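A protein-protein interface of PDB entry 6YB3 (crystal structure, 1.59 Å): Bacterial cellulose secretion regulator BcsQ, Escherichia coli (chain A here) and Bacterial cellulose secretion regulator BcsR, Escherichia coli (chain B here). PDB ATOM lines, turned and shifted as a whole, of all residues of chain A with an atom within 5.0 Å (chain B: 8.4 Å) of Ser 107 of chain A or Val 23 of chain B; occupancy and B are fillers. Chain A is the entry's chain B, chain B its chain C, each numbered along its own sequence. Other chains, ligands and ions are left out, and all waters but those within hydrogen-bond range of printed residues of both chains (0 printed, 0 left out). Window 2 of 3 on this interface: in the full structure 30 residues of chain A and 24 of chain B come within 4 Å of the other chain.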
ATOM      1  N   SER A 103      -0.796  24.238  35.238  1.00  0.00           N
ATOM      2  CA  SER A 103      -1.104  23.850  33.863  1.00  0.00           C
ATOM      3  C   SER A 103      -1.119  25.029  32.901  1.00  0.00           C
ATOM      4  O   SER A 103      -0.906  24.830  31.698  1.00  0.00           O
ATOM      5  CB  SER A 103      -2.464  23.147  33.794  1.00  0.00           C
ATOM      6  OG  SER A 103      -2.476  21.970  34.579  1.00  0.00           O
ATOM      7  N   ASP A 104      -1.369  26.246  33.395  1.00  0.00           N
ATOM      8  CA  ASP A 104      -1.456  27.408  32.512  1.00  0.00           C
ATOM      9  C   ASP A 104      -0.164  27.638  31.741  1.00  0.00           C
ATOM     10  O   ASP A 104      -0.190  28.225  30.650  1.00  0.00           O
ATOM     11  CB  ASP A 104      -1.800  28.665  33.310  1.00  0.00           C
ATOM     12  CG  ASP A 104      -3.298  28.869  33.485  1.00  0.00           C
ATOM     13  OD1 ASP A 104      -4.093  27.938  33.211  1.00  0.00           O
ATOM     14  OD2 ASP A 104      -3.675  29.983  33.901  1.00  0.00           O
ATOM     15  N   ILE A 105       0.974  27.203  32.289  1.00  0.00           N
ATOM     16  CA  ILE A 105       2.251  27.383  31.602  1.00  0.00           C
ATOM     17  C   ILE A 105       2.257  26.641  30.273  1.00  0.00           C
ATOM     18  O   ILE A 105       2.906  27.077  29.311  1.00  0.00           O
ATOM     19  CB  ILE A 105       3.430  26.944  32.507  1.00  0.00           C
ATOM     20  CG1 ILE A 105       4.758  27.509  31.992  1.00  0.00           C
ATOM     21  CG2 ILE A 105       3.568  25.444  32.567  1.00  0.00           C
ATOM     22  CD1 ILE A 105       4.815  29.018  31.998  1.00  0.00           C
ATOM     23  N   CYS A 106       1.551  25.513  30.185  1.00  0.00           N
ATOM     24  CA  CYS A 106       1.532  24.751  28.940  1.00  0.00           C
ATOM     25  C   CYS A 106       0.866  25.532  27.818  1.00  0.00           C
ATOM     26  O   CYS A 106       1.389  25.594  26.700  1.00  0.00           O
ATOM     27  CB  CYS A 106       0.822  23.423  29.146  1.00  0.00           C
ATOM     28  SG  CYS A 106       1.747  22.358  30.188  1.00  0.00           S
ATOM     29  N   SER A 107      -0.302  26.117  28.087  1.00  0.00           N
ATOM     30  CA  SER A 107      -0.948  26.909  27.045  1.00  0.00           C
ATOM     31  C   SER A 107      -0.118  28.142  26.708  1.00  0.00           C
ATOM     32  O   SER A 107      -0.048  28.543  25.537  1.00  0.00           O
ATOM     33  CB  SER A 107      -2.368  27.302  27.466  1.00  0.00           C
ATOM     34  OG  SER A 107      -2.362  28.141  28.608  1.00  0.00           O
ATOM     35  N   GLY A 108       0.560  28.723  27.702  1.00  0.00           N
ATOM     36  CA  GLY A 108       1.350  29.913  27.441  1.00  0.00           C
ATOM     37  C   GLY A 108       2.563  29.625  26.576  1.00  0.00           C
ATOM     38  O   GLY A 108       2.909  30.419  25.689  1.00  0.00           O
ATOM     39  N   LEU A 109       3.238  28.495  26.830  1.00  0.00           N
ATOM     40  CA  LEU A 109       4.369  28.108  25.990  1.00  0.00           C
ATOM     41  C   LEU A 109       3.907  27.631  24.616  1.00  0.00           C
ATOM     42  O   LEU A 109       4.609  27.844  23.620  1.00  0.00           O
ATOM     43  CB  LEU A 109       5.214  27.039  26.696  1.00  0.00           C
ATOM     44  CG  LEU A 109       5.943  27.553  27.940  1.00  0.00           C
ATOM     45  CD1 LEU A 109       6.745  26.441  28.626  1.00  0.00           C
ATOM     46  CD2 LEU A 109       6.849  28.733  27.609  1.00  0.00           C
ATOM     47  N   GLN A 110       2.725  27.013  24.532  1.00  0.00           N
ATOM     48  CA  GLN A 110       2.172  26.655  23.228  1.00  0.00           C
ATOM     49  C   GLN A 110       1.917  27.895  22.375  1.00  0.00           C
ATOM     50  O   GLN A 110       2.196  27.897  21.167  1.00  0.00           O
ATOM     51  CB  GLN A 110       0.881  25.855  23.414  1.00  0.00           C
ATOM     52  CG  GLN A 110       0.453  25.078  22.178  1.00  0.00           C
ATOM     53  CD  GLN A 110       1.232  23.781  22.007  1.00  0.00           C
ATOM     54  OE1 GLN A 110       2.433  23.724  22.265  1.00  0.00           O
ATOM     55  NE2 GLN A 110       0.546  22.731  21.574  1.00  0.00           N
ATOM     56  N   GLN A 111       1.366  28.952  22.985  1.00  0.00           N
ATOM     57  CA  GLN A 111       1.204  30.223  22.284  1.00  0.00           C
ATOM     58  C   GLN A 111       2.541  30.778  21.836  1.00  0.00           C
ATOM     59  O   GLN A 111       2.670  31.274  20.713  1.00  0.00           O
ATOM     60  CB  GLN A 111       0.533  31.250  23.182  1.00  0.00           C
ATOM     61  CG  GLN A 111      -0.889  30.989  23.530  1.00  0.00           C
ATOM     62  CD  GLN A 111      -1.389  32.063  24.455  1.00  0.00           C
ATOM     63  OE1 GLN A 111      -1.020  32.099  25.628  1.00  0.00           O
ATOM     64  NE2 GLN A 111      -2.187  32.983  23.924  1.00  0.00           N
ATOM     65  N   LEU A 139       5.245  19.260  25.419  1.00  0.00           N
ATOM     66  CA  LEU A 139       5.423  20.404  24.531  1.00  0.00           C
ATOM     67  C   LEU A 139       6.728  20.348  23.749  1.00  0.00           C
ATOM     68  O   LEU A 139       6.894  21.122  22.798  1.00  0.00           O
ATOM     69  CB  LEU A 139       5.397  21.706  25.329  1.00  0.00           C
ATOM     70  CG  LEU A 139       4.150  22.056  26.132  1.00  0.00           C
ATOM     71  CD1 LEU A 139       4.431  23.244  27.028  1.00  0.00           C
ATOM     72  CD2 LEU A 139       3.020  22.372  25.189  1.00  0.00           C
ATOM     73  N   GLN B  19      -1.246  11.792  29.116  1.00  0.00           N
ATOM     74  CA  GLN B  19      -2.261  12.581  28.427  1.00  0.00           C
ATOM     75  C   GLN B  19      -2.276  13.992  29.003  1.00  0.00           C
ATOM     76  O   GLN B  19      -2.452  14.172  30.213  1.00  0.00           O
ATOM     77  CB  GLN B  19      -3.640  11.924  28.545  1.00  0.00           C
ATOM     78  CG  GLN B  19      -3.995  11.441  29.947  1.00  0.00           C
ATOM     79  CD  GLN B  19      -5.329  10.714  29.996  1.00  0.00           C
ATOM     80  OE1 GLN B  19      -5.758  10.108  29.013  1.00  0.00           O
ATOM     81  NE2 GLN B  19      -5.993  10.774  31.146  1.00  0.00           N
ATOM     82  N   ASN B  20      -2.086  14.987  28.138  1.00  0.00           N
ATOM     83  CA  ASN B  20      -2.104  16.400  28.515  1.00  0.00           C
ATOM     84  C   ASN B  20      -3.323  17.038  27.853  1.00  0.00           C
ATOM     85  O   ASN B  20      -3.231  17.663  26.794  1.00  0.00           O
ATOM     86  CB  ASN B  20      -0.790  17.101  28.103  1.00  0.00           C
ATOM     87  CG  ASN B  20      -0.727  18.553  28.554  1.00  0.00           C
ATOM     88  OD1 ASN B  20      -1.562  19.015  29.331  1.00  0.00           O
ATOM     89  ND2 ASN B  20       0.279  19.277  28.072  1.00  0.00           N
ATOM     90  N   ASP B  21      -4.482  16.878  28.495  1.00  0.00           N
ATOM     91  CA  ASP B  21      -5.726  17.373  27.920  1.00  0.00           C
ATOM     92  C   ASP B  21      -5.760  18.891  27.816  1.00  0.00           C
ATOM     93  O   ASP B  21      -6.499  19.425  26.982  1.00  0.00           O
ATOM     94  CB  ASP B  21      -6.919  16.889  28.749  1.00  0.00           C
ATOM     95  CG  ASP B  21      -7.126  15.389  28.653  1.00  0.00           C
ATOM     96  OD1 ASP B  21      -7.069  14.849  27.529  1.00  0.00           O
ATOM     97  OD2 ASP B  21      -7.343  14.749  29.704  1.00  0.00           O
ATOM     98  N   ILE B  22      -4.971  19.600  28.630  1.00  0.00           N
ATOM     99  CA  ILE B  22      -5.091  21.052  28.695  1.00  0.00           C
ATOM    100  C   ILE B  22      -4.597  21.725  27.418  1.00  0.00           C
ATOM    101  O   ILE B  22      -4.988  22.863  27.131  1.00  0.00           O
ATOM    102  CB  ILE B  22      -4.360  21.591  29.941  1.00  0.00           C
ATOM    103  CG1 ILE B  22      -5.032  22.872  30.435  1.00  0.00           C
ATOM    104  CG2 ILE B  22      -2.889  21.839  29.659  1.00  0.00           C
ATOM    105  CD1 ILE B  22      -6.470  22.672  30.860  1.00  0.00           C
ATOM    106  N   VAL B  23      -3.742  21.054  26.642  1.00  0.00           N
ATOM    107  CA  VAL B  23      -3.340  21.525  25.322  1.00  0.00           C
ATOM    108  C   VAL B  23      -3.556  20.468  24.246  1.00  0.00           C
ATOM    109  O   VAL B  23      -3.211  20.698  23.087  1.00  0.00           O
ATOM    110  CB  VAL B  23      -1.872  22.016  25.329  1.00  0.00           C
ATOM    111  CG1 VAL B  23      -1.528  22.806  24.080  1.00  0.00           C
ATOM    112  CG2 VAL B  23      -1.633  22.909  26.520  1.00  0.00           C
ATOM    113  N   ALA B  24      -4.151  19.325  24.592  1.00  0.00           N
ATOM    114  CA  ALA B  24      -4.439  18.239  23.652  1.00  0.00           C
ATOM    115  C   ALA B  24      -3.148  17.671  23.055  1.00  0.00           C
ATOM    116  O   ALA B  24      -2.953  17.627  21.838  1.00  0.00           O
ATOM    117  CB  ALA B  24      -5.410  18.694  22.555  1.00  0.00           C
ATOM    118  N   LEU B  25      -2.268  17.225  23.946  1.00  0.00           N
ATOM    119  CA  LEU B  25      -1.000  16.625  23.568  1.00  0.00           C
ATOM    120  C   LEU B  25      -0.787  15.349  24.368  1.00  0.00           C
ATOM    121  O   LEU B  25      -1.335  15.177  25.460  1.00  0.00           O
ATOM    122  CB  LEU B  25       0.172  17.585  23.801  1.00  0.00           C
ATOM    123  CG  LEU B  25       0.093  18.935  23.091  1.00  0.00           C
ATOM    124  CD1 LEU B  25       1.178  19.845  23.609  1.00  0.00           C
ATOM    125  CD2 LEU B  25       0.218  18.757  21.588  1.00  0.00           C
ATOM    126  N   LYS B  26       0.022  14.453  23.810  1.00  0.00           N
ATOM    127  CA  LYS B  26       0.392  13.213  24.473  1.00  0.00           C
ATOM    128  C   LYS B  26       1.910  13.105  24.553  1.00  0.00           C
ATOM    129  O   LYS B  26       2.636  13.622  23.698  1.00  0.00           O
ATOM    130  CB  LYS B  26      -0.199  11.991  23.749  1.00  0.00           C
ATOM    131  CG  LYS B  26      -1.715  11.890  23.864  1.00  0.00           C
ATOM    132  CD  LYS B  26      -2.270  10.649  23.175  1.00  0.00           C
ATOM    133  CE  LYS B  26      -3.792  10.608  23.282  1.00  0.00           C
ATOM    134  NZ  LYS B  26      -4.398   9.450  22.565  1.00  0.00           N
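O of Asp 104 of chain A is in hydrogen-bond range of OG of Ser 107 of chain A, at 3.0 Å. The backbone carbonyl oxygen (O) of Leu 25 of chain B lies within hydrogen-bond range of the backbone NH (N) of Asn 20 of chain B (2.8 Å).
Among the printed residues, merely in contact across the chains: Gln 110 of chain A with Val 23 of chain B, Leu 139 of chain A with Leu 25 of chain B, Gln 110 of chain A with Leu 25 of chain B, Cys 106 of chain A with Val 23 of chain B and Ser 107 of chain A with Val 23 of chain B.
Ser 107 of chain A touches just one residue of chain B: Val 23 (3.8 Å). No residue of chain B comes within 4 Å of Gly 108 of chain A. Printed residues of chain B within 4 Å of Gln 110 of chain A: Val 23 and Leu 25. Printed residues of chain B within 4 Å of Cys 106 of chain A: Val 23 (3.6 Å). Of the printed residues of chain B, Leu 139 of chain A touches Leu 25. Printed residues of chain A within 4 Å of Leu 25 of chain B: Gln 110 and Leu 139. The nearest residue of chain B that does not touch Ser 107 of chain A is Ile 22 of chain B (5.2 Å). The nearest printed residue of chain A that does not touch Leu 25 of chain B is Cys 106 of chain A (6.5 Å).
Printed residues of chain A that touch a printed residue of chain B: Cys 106, Ser 107, Gln 110 and Leu 139. Of the 8 printed residues of chain B, 2 touch a printed residue of chain A. Printed residues of chain B that touch a printed residue of chain A: Val 23 and Leu 25. Hydrophobic or aromatic side chains of chain B that line the printed part of chain A: Val 23 and Leu 25.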
